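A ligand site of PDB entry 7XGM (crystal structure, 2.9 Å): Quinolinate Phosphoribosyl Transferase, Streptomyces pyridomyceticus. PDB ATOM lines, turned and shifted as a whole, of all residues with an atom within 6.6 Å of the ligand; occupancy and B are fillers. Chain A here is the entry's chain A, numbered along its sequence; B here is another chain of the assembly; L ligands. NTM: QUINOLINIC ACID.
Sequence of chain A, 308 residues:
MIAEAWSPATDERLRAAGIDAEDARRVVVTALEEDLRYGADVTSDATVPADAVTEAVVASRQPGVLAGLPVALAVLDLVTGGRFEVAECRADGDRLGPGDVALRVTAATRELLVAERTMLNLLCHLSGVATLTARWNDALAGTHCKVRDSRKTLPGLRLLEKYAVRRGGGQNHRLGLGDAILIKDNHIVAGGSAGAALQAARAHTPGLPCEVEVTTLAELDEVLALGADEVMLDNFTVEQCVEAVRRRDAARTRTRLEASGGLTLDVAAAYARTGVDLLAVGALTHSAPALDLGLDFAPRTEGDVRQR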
ATOM      1  N   ARG A 148     -14.302  -4.857   4.761  1.00  0.00           N
ATOM      2  CA  ARG A 148     -15.190  -5.726   5.510  1.00  0.00           C
ATOM      3  C   ARG A 148     -15.531  -5.087   6.837  1.00  0.00           C
ATOM      4  O   ARG A 148     -14.804  -4.244   7.364  1.00  0.00           O
ATOM      5  CB  ARG A 148     -14.588  -7.100   5.752  1.00  0.00           C
ATOM      6  CG  ARG A 148     -14.304  -7.867   4.508  1.00  0.00           C
ATOM      7  CD  ARG A 148     -13.266  -8.877   4.825  1.00  0.00           C
ATOM      8  NE  ARG A 148     -13.808 -10.220   4.885  1.00  0.00           N
ATOM      9  CZ  ARG A 148     -13.253 -11.217   5.551  1.00  0.00           C
ATOM     10  NH1 ARG A 148     -12.237 -11.017   6.366  1.00  0.00           N
ATOM     11  NH2 ARG A 148     -13.724 -12.455   5.395  1.00  0.00           N
ATOM     12  N   ASP A 149     -16.662  -5.522   7.368  1.00  0.00           N
ATOM     13  CA  ASP A 149     -17.118  -5.080   8.681  1.00  0.00           C
ATOM     14  C   ASP A 149     -16.544  -5.992   9.760  1.00  0.00           C
ATOM     15  O   ASP A 149     -15.445  -6.536   9.609  1.00  0.00           O
ATOM     16  CB  ASP A 149     -18.638  -5.064   8.688  1.00  0.00           C
ATOM     17  CG  ASP A 149     -19.224  -6.336   8.104  1.00  0.00           C
ATOM     18  OD1 ASP A 149     -18.524  -7.376   8.159  1.00  0.00           O
ATOM     19  OD2 ASP A 149     -20.358  -6.294   7.577  1.00  0.00           O
ATOM     20  N   SER A 150     -17.285  -6.200  10.851  1.00  0.00           N
ATOM     21  CA  SER A 150     -16.750  -6.966  11.967  1.00  0.00           C
ATOM     22  C   SER A 150     -17.914  -7.369  12.857  1.00  0.00           C
ATOM     23  O   SER A 150     -19.071  -7.369  12.431  1.00  0.00           O
ATOM     24  CB  SER A 150     -15.706  -6.143  12.733  1.00  0.00           C
ATOM     25  OG  SER A 150     -16.318  -5.001  13.292  1.00  0.00           O
ATOM     26  N   ARG A 151     -17.599  -7.744  14.093  1.00  0.00           N
ATOM     27  CA  ARG A 151     -18.597  -8.038  15.091  1.00  0.00           C
ATOM     28  C   ARG A 151     -18.886  -6.832  15.969  1.00  0.00           C
ATOM     29  O   ARG A 151     -19.711  -6.920  16.882  1.00  0.00           O
ATOM     30  CB  ARG A 151     -18.156  -9.248  15.935  1.00  0.00           C
ATOM     31  CG  ARG A 151     -18.581 -10.577  15.333  1.00  0.00           C
ATOM     32  CD  ARG A 151     -17.883 -11.777  15.972  1.00  0.00           C
ATOM     33  NE  ARG A 151     -18.218 -11.927  17.381  1.00  0.00           N
ATOM     34  CZ  ARG A 151     -17.381 -11.691  18.395  1.00  0.00           C
ATOM     35  NH1 ARG A 151     -16.104 -11.374  18.201  1.00  0.00           N
ATOM     36  NH2 ARG A 151     -17.839 -11.793  19.633  1.00  0.00           N
ATOM     37  N   LYS A 152     -18.239  -5.716  15.697  1.00  0.00           N
ATOM     38  CA  LYS A 152     -18.450  -4.498  16.466  1.00  0.00           C
ATOM     39  C   LYS A 152     -19.701  -3.787  15.945  1.00  0.00           C
ATOM     40  O   LYS A 152     -19.662  -2.686  15.396  1.00  0.00           O
ATOM     41  CB  LYS A 152     -17.209  -3.641  16.390  1.00  0.00           C
ATOM     42  CG  LYS A 152     -15.969  -4.343  16.951  1.00  0.00           C
ATOM     43  CD  LYS A 152     -14.831  -3.384  17.251  1.00  0.00           C
ATOM     44  CE  LYS A 152     -13.493  -4.026  16.991  1.00  0.00           C
ATOM     45  NZ  LYS A 152     -12.426  -3.228  17.641  1.00  0.00           N
ATOM     46  N   THR A 153     -20.834  -4.467  16.105  1.00  0.00           N
ATOM     47  CA  THR A 153     -22.124  -4.011  15.642  1.00  0.00           C
ATOM     48  C   THR A 153     -22.941  -3.559  16.842  1.00  0.00           C
ATOM     49  O   THR A 153     -22.584  -3.833  17.991  1.00  0.00           O
ATOM     50  CB  THR A 153     -22.842  -5.110  14.840  1.00  0.00           C
ATOM     51  OG1 THR A 153     -23.257  -6.186  15.703  1.00  0.00           O
ATOM     52  CG2 THR A 153     -21.904  -5.670  13.764  1.00  0.00           C
ATOM     53  N   LYS A 162     -25.090  -5.826   8.915  1.00  0.00           N
ATOM     54  CA  LYS A 162     -24.369  -6.580   7.903  1.00  0.00           C
ATOM     55  C   LYS A 162     -25.031  -6.417   6.527  1.00  0.00           C
ATOM     56  O   LYS A 162     -24.354  -6.176   5.517  1.00  0.00           O
ATOM     57  CB  LYS A 162     -24.290  -8.051   8.308  1.00  0.00           C
ATOM     58  CG  LYS A 162     -23.525  -8.338   9.590  1.00  0.00           C
ATOM     59  CD  LYS A 162     -22.020  -8.338   9.366  1.00  0.00           C
ATOM     60  CE  LYS A 162     -21.230  -8.855  10.581  1.00  0.00           C
ATOM     61  NZ  LYS A 162     -19.747  -8.932  10.287  1.00  0.00           N
ATOM     62  N   HIS A 173     -17.839  -9.937   7.465  1.00  0.00           N
ATOM     63  CA  HIS A 173     -16.980 -10.887   8.140  1.00  0.00           C
ATOM     64  C   HIS A 173     -17.893 -11.974   8.725  1.00  0.00           C
ATOM     65  O   HIS A 173     -19.061 -12.104   8.334  1.00  0.00           O
ATOM     66  CB  HIS A 173     -16.150 -10.144   9.176  1.00  0.00           C
ATOM     67  CG  HIS A 173     -14.831 -10.788   9.436  1.00  0.00           C
ATOM     68  ND1 HIS A 173     -13.629 -10.176   9.123  1.00  0.00           N
ATOM     69  CD2 HIS A 173     -14.505 -11.981   9.990  1.00  0.00           C
ATOM     70  CE1 HIS A 173     -12.637 -10.963   9.472  1.00  0.00           C
ATOM     71  NE2 HIS A 173     -13.141 -12.069   9.997  1.00  0.00           N
ATOM     72  N   ARG A 174     -17.384 -12.792   9.637  1.00  0.00           N
ATOM     73  CA  ARG A 174     -18.245 -13.772  10.277  1.00  0.00           C
ATOM     74  C   ARG A 174     -19.380 -13.076  11.021  1.00  0.00           C
ATOM     75  O   ARG A 174     -19.286 -11.894  11.375  1.00  0.00           O
ATOM     76  CB  ARG A 174     -17.448 -14.650  11.227  1.00  0.00           C
ATOM     77  CG  ARG A 174     -16.762 -13.873  12.306  1.00  0.00           C
ATOM     78  CD  ARG A 174     -16.042 -14.768  13.262  1.00  0.00           C
ATOM     79  NE  ARG A 174     -15.387 -14.015  14.323  1.00  0.00           N
ATOM     80  CZ  ARG A 174     -14.918 -14.556  15.437  1.00  0.00           C
ATOM     81  NH1 ARG A 174     -15.037 -15.855  15.681  1.00  0.00           N
ATOM     82  NH2 ARG A 174     -14.342 -13.778  16.337  1.00  0.00           N
ATOM     83  N   LEU A 175     -20.458 -13.806  11.252  1.00  0.00           N
ATOM     84  CA  LEU A 175     -21.602 -13.271  11.971  1.00  0.00           C
ATOM     85  C   LEU A 175     -21.566 -13.543  13.485  1.00  0.00           C
ATOM     86  O   LEU A 175     -22.287 -12.880  14.233  1.00  0.00           O
ATOM     87  CB  LEU A 175     -22.908 -13.829  11.390  1.00  0.00           C
ATOM     88  CG  LEU A 175     -23.086 -13.754   9.877  1.00  0.00           C
ATOM     89  CD1 LEU A 175     -24.439 -14.290   9.480  1.00  0.00           C
ATOM     90  CD2 LEU A 175     -22.919 -12.336   9.385  1.00  0.00           C
ATOM     91  N   GLY A 176     -20.747 -14.479  13.944  1.00  0.00           N
ATOM     92  CA  GLY A 176     -20.743 -14.786  15.360  1.00  0.00           C
ATOM     93  C   GLY A 176     -19.468 -15.478  15.778  1.00  0.00           C
ATOM     94  O   GLY A 176     -18.489 -15.512  15.040  1.00  0.00           O
ATOM     95  N   LEU A 177     -19.494 -16.018  16.986  1.00  0.00           N
ATOM     96  CA  LEU A 177     -18.348 -16.735  17.517  1.00  0.00           C
ATOM     97  C   LEU A 177     -18.225 -18.147  16.959  1.00  0.00           C
ATOM     98  O   LEU A 177     -17.145 -18.751  17.087  1.00  0.00           O
ATOM     99  CB  LEU A 177     -18.441 -16.802  19.039  1.00  0.00           C
ATOM    100  CG  LEU A 177     -18.098 -15.496  19.730  1.00  0.00           C
ATOM    101  CD1 LEU A 177     -18.261 -15.642  21.206  1.00  0.00           C
ATOM    102  CD2 LEU A 177     -16.681 -15.098  19.396  1.00  0.00           C
ATOM    103  N   LEU A 182     -11.490 -16.970  14.384  1.00  0.00           N
ATOM    104  CA  LEU A 182     -10.626 -15.793  14.306  1.00  0.00           C
ATOM    105  C   LEU A 182      -9.820 -15.739  15.601  1.00  0.00           C
ATOM    106  O   LEU A 182     -10.371 -15.430  16.666  1.00  0.00           O
ATOM    107  CB  LEU A 182     -11.452 -14.521  14.088  1.00  0.00           C
ATOM    108  CG  LEU A 182     -10.720 -13.166  14.121  1.00  0.00           C
ATOM    109  CD1 LEU A 182      -9.571 -13.105  13.113  1.00  0.00           C
ATOM    110  CD2 LEU A 182     -11.690 -12.039  13.884  1.00  0.00           C
ATOM    111  N   LYS A 184      -7.445 -14.225  18.221  1.00  0.00           N
ATOM    112  CA  LYS A 184      -7.244 -12.839  18.617  1.00  0.00           C
ATOM    113  C   LYS A 184      -6.067 -12.714  19.581  1.00  0.00           C
ATOM    114  O   LYS A 184      -5.459 -13.701  20.004  1.00  0.00           O
ATOM    115  CB  LYS A 184      -8.528 -12.271  19.231  1.00  0.00           C
ATOM    116  CG  LYS A 184      -9.733 -12.259  18.264  1.00  0.00           C
ATOM    117  CD  LYS A 184     -11.029 -11.783  18.949  1.00  0.00           C
ATOM    118  CE  LYS A 184     -11.923 -11.036  17.967  1.00  0.00           C
ATOM    119  NZ  LYS A 184     -11.115 -10.137  17.092  1.00  0.00           N
ATOM    120  N   GLU A 211      -8.901 -17.649  10.405  1.00  0.00           N
ATOM    121  CA  GLU A 211      -8.074 -16.454  10.291  1.00  0.00           C
ATOM    122  C   GLU A 211      -7.388 -16.184  11.624  1.00  0.00           C
ATOM    123  O   GLU A 211      -7.981 -16.372  12.682  1.00  0.00           O
ATOM    124  CB  GLU A 211      -8.939 -15.250   9.876  1.00  0.00           C
ATOM    125  CG  GLU A 211      -8.169 -13.970   9.704  1.00  0.00           C
ATOM    126  CD  GLU A 211      -9.037 -12.816   9.233  1.00  0.00           C
ATOM    127  OE1 GLU A 211     -10.280 -12.930   9.291  1.00  0.00           O
ATOM    128  OE2 GLU A 211      -8.484 -11.789   8.793  1.00  0.00           O
ATOM    129  N   GLU A 213      -4.951 -13.366  13.894  1.00  0.00           N
ATOM    130  CA  GLU A 213      -4.695 -11.941  14.024  1.00  0.00           C
ATOM    131  C   GLU A 213      -3.334 -11.763  14.687  1.00  0.00           C
ATOM    132  O   GLU A 213      -3.107 -12.265  15.796  1.00  0.00           O
ATOM    133  CB  GLU A 213      -5.823 -11.294  14.819  1.00  0.00           C
ATOM    134  CG  GLU A 213      -5.670  -9.859  15.219  1.00  0.00           C
ATOM    135  CD  GLU A 213      -6.622  -9.508  16.363  1.00  0.00           C
ATOM    136  OE1 GLU A 213      -7.856  -9.406  16.095  1.00  0.00           O
ATOM    137  OE2 GLU A 213      -6.127  -9.380  17.521  1.00  0.00           O
ATOM    138  N   MET A 232      -4.740 -11.522   9.765  1.00  0.00           N
ATOM    139  CA  MET A 232      -5.176 -10.175  10.091  1.00  0.00           C
ATOM    140  C   MET A 232      -4.031  -9.441  10.776  1.00  0.00           C
ATOM    141  O   MET A 232      -3.514  -9.894  11.800  1.00  0.00           O
ATOM    142  CB  MET A 232      -6.417 -10.211  10.979  1.00  0.00           C
ATOM    143  CG  MET A 232      -7.074  -8.869  11.127  1.00  0.00           C
ATOM    144  SD  MET A 232      -8.383  -8.865  12.347  1.00  0.00           S
ATOM    145  CE  MET A 232      -9.660  -9.756  11.454  1.00  0.00           C
ATOM    146  N   GLU A 258      -5.278  -9.126   5.999  1.00  0.00           N
ATOM    147  CA  GLU A 258      -6.368  -8.230   6.318  1.00  0.00           C
ATOM    148  C   GLU A 258      -5.868  -7.236   7.356  1.00  0.00           C
ATOM    149  O   GLU A 258      -5.328  -7.633   8.380  1.00  0.00           O
ATOM    150  CB  GLU A 258      -7.586  -9.002   6.815  1.00  0.00           C
ATOM    151  CG  GLU A 258      -8.735  -8.113   7.164  1.00  0.00           C
ATOM    152  CD  GLU A 258     -10.048  -8.876   7.214  1.00  0.00           C
ATOM    153  OE1 GLU A 258     -10.025 -10.066   7.590  1.00  0.00           O
ATOM    154  OE2 GLU A 258     -11.103  -8.302   6.867  1.00  0.00           O
ATOM    155  N   SER A 260      -6.468  -4.361  10.182  1.00  0.00           N
ATOM    156  CA  SER A 260      -7.518  -3.947  11.097  1.00  0.00           C
ATOM    157  C   SER A 260      -6.893  -3.270  12.296  1.00  0.00           C
ATOM    158  O   SER A 260      -5.795  -3.623  12.730  1.00  0.00           O
ATOM    159  CB  SER A 260      -8.370  -5.129  11.532  1.00  0.00           C
ATOM    160  OG  SER A 260      -9.520  -4.670  12.230  1.00  0.00           O
ATOM    161  N   ALA A 280     -10.586  -4.403   7.467  1.00  0.00           N
ATOM    162  CA  ALA A 280     -11.680  -4.699   8.380  1.00  0.00           C
ATOM    163  C   ALA A 280     -11.936  -3.465   9.230  1.00  0.00           C
ATOM    164  O   ALA A 280     -11.042  -3.012   9.960  1.00  0.00           O
ATOM    165  CB  ALA A 280     -11.380  -5.923   9.242  1.00  0.00           C
ATOM    166  N   VAL A 281     -13.132  -2.894   9.117  1.00  0.00           N
ATOM    167  CA  VAL A 281     -13.429  -1.592   9.685  1.00  0.00           C
ATOM    168  C   VAL A 281     -14.635  -1.731  10.606  1.00  0.00           C
ATOM    169  O   VAL A 281     -15.761  -1.959  10.144  1.00  0.00           O
ATOM    170  CB  VAL A 281     -13.679  -0.535   8.597  1.00  0.00           C
ATOM    171  CG1 VAL A 281     -14.012   0.800   9.230  1.00  0.00           C
ATOM    172  CG2 VAL A 281     -12.476  -0.415   7.687  1.00  0.00           C
ATOM    173  N   GLY A 282     -14.396  -1.581  11.902  1.00  0.00           N
ATOM    174  CA  GLY A 282     -15.501  -1.579  12.854  1.00  0.00           C
ATOM    175  C   GLY A 282     -16.356  -0.339  12.719  1.00  0.00           C
ATOM    176  O   GLY A 282     -17.578  -0.410  12.892  1.00  0.00           O
ATOM    177  N   GLU B 116     -16.745 -10.775  26.036  1.00  0.00           N
ATOM    178  CA  GLU B 116     -15.912  -9.612  25.713  1.00  0.00           C
ATOM    179  C   GLU B 116     -16.577  -8.691  24.706  1.00  0.00           C
ATOM    180  O   GLU B 116     -16.655  -7.472  24.916  1.00  0.00           O
ATOM    181  CB  GLU B 116     -14.557 -10.086  25.178  1.00  0.00           C
ATOM    182  CG  GLU B 116     -13.688  -8.963  24.664  1.00  0.00           C
ATOM    183  CD  GLU B 116     -12.388  -9.439  23.987  1.00  0.00           C
ATOM    184  OE1 GLU B 116     -12.078 -10.652  24.062  1.00  0.00           O
ATOM    185  OE2 GLU B 116     -11.678  -8.574  23.379  1.00  0.00           O
ATOM    186  N   ARG B 117     -17.039  -9.239  23.595  1.00  0.00           N
ATOM    187  CA  ARG B 117     -17.489  -8.380  22.516  1.00  0.00           C
ATOM    188  C   ARG B 117     -18.871  -7.772  22.810  1.00  0.00           C
ATOM    189  O   ARG B 117     -19.113  -6.602  22.516  1.00  0.00           O
ATOM    190  CB  ARG B 117     -17.448  -9.181  21.207  1.00  0.00           C
ATOM    191  CG  ARG B 117     -17.968  -8.493  19.955  1.00  0.00           C
ATOM    192  CD  ARG B 117     -17.477  -7.074  19.789  1.00  0.00           C
ATOM    193  NE  ARG B 117     -16.033  -6.970  19.772  1.00  0.00           N
ATOM    194  CZ  ARG B 117     -15.372  -5.873  20.138  1.00  0.00           C
ATOM    195  NH1 ARG B 117     -16.033  -4.757  20.474  1.00  0.00           N
ATOM    196  NH2 ARG B 117     -14.044  -5.900  20.189  1.00  0.00           N
ATOM    197  N   ASN B 121     -19.343  -3.794  22.965  1.00  0.00           N
ATOM    198  CA  ASN B 121     -20.289  -3.135  22.064  1.00  0.00           C
ATOM    199  C   ASN B 121     -21.258  -2.257  22.839  1.00  0.00           C
ATOM    200  O   ASN B 121     -21.631  -1.174  22.374  1.00  0.00           O
ATOM    201  CB  ASN B 121     -21.036  -4.166  21.224  1.00  0.00           C
ATOM    202  CG  ASN B 121     -20.184  -4.753  20.125  1.00  0.00           C
ATOM    203  OD1 ASN B 121     -19.092  -4.260  19.833  1.00  0.00           O
ATOM    204  ND2 ASN B 121     -20.667  -5.820  19.505  1.00  0.00           N
HETATM  205  N1  NTM L   1     -12.915  -7.165  13.974  1.00  0.00           N
HETATM  206  C2  NTM L   1     -13.557  -8.154  14.622  1.00  0.00           C
HETATM  207  C3  NTM L   1     -13.915  -9.323  13.954  1.00  0.00           C
HETATM  208  C4  NTM L   1     -13.607  -9.448  12.640  1.00  0.00           C
HETATM  209  C5  NTM L   1     -12.956  -8.451  12.000  1.00  0.00           C
HETATM  210  C6  NTM L   1     -12.605  -7.300  12.670  1.00  0.00           C
HETATM  211  C7  NTM L   1     -13.915  -7.915  16.091  1.00  0.00           C
HETATM  212  O1  NTM L   1     -13.032  -8.040  16.999  1.00  0.00           O
HETATM  213  O2  NTM L   1     -15.117  -7.567  16.336  1.00  0.00           O
HETATM  214  C8  NTM L   1     -14.644 -10.482  14.619  1.00  0.00           C
HETATM  215  O3  NTM L   1     -14.307 -10.832  15.788  1.00  0.00           O
HETATM  216  O4  NTM L   1     -15.551 -11.100  13.970  1.00  0.00           O
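The side-chain amino group (NZ) of Lys 184 is in salt-bridge range of the side-chain carboxylate (OE1) of Glu 213 (3.5 Å). The side-chain amino group (NZ) of Lys 162 lies within hydrogen-bond range of the backbone carbonyl oxygen (O) of Arg 174 (3.2 Å). The backbone carbonyl oxygen of Arg 151 lies within hydrogen-bond range of the side-chain amide nitrogen of Asn 121 of chain B, 3.0 Å away. OG of Ser 150 lies within hydrogen-bond range of N of Lys 152, 3.2 Å away. The side-chain carboxylate of Glu 211 lies within hydrogen-bond range of a ring nitrogen (NE2) of His 173 (3.1 Å). The guanidinium group of Arg 117 of chain B is in hydrogen-bond range of the side-chain amide oxygen of Asn 121 of chain B, 3.2 Å away. The backbone carbonyl oxygen (O) of Ala 280 sits at hydrogen-bond distance from the side-chain hydroxyl (OG) of Ser 260, 3.2 Å away. The side-chain carboxylate (OD1) of Asp 149 lies within salt-bridge range of the side-chain amino group (NZ) of Lys 162.
Residues that only touch the ligand: Ser 150, Lys 152, Leu 182, His 173, Met 232, Ala 280 and Asp 149. Hydrophobic or aromatic side chains that line the ligand: His 173, Leu 182, Met 232 and Ala 280. Within 4 Å of the ligand: Asp 149, Ser 150, Arg 151, Lys 152, His 173, Arg 174, Leu 182, Lys 184, Met 232, Ala 280 and Arg 117 of chain B. The nearest printed residue that does not touch the ligand is Ser 260 (4.1 Å).
NZ of Lys 184 is in salt-bridge range of O1 of the ligand (2.8 Å). The guanidinium group of Arg 174 lies within salt-bridge range of an oxygen (O4) of the ligand. O2 of the ligand is in hydrogen-bond range of N of Arg 151, at 3.4 Å. NH1 of Arg 151 lies within salt-bridge range of O3 of the ligand (3.1 Å). The guanidinium group (NE) of Arg 117 of chain B lies within salt-bridge range of an oxygen (O2) of the ligand (3.6 Å).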
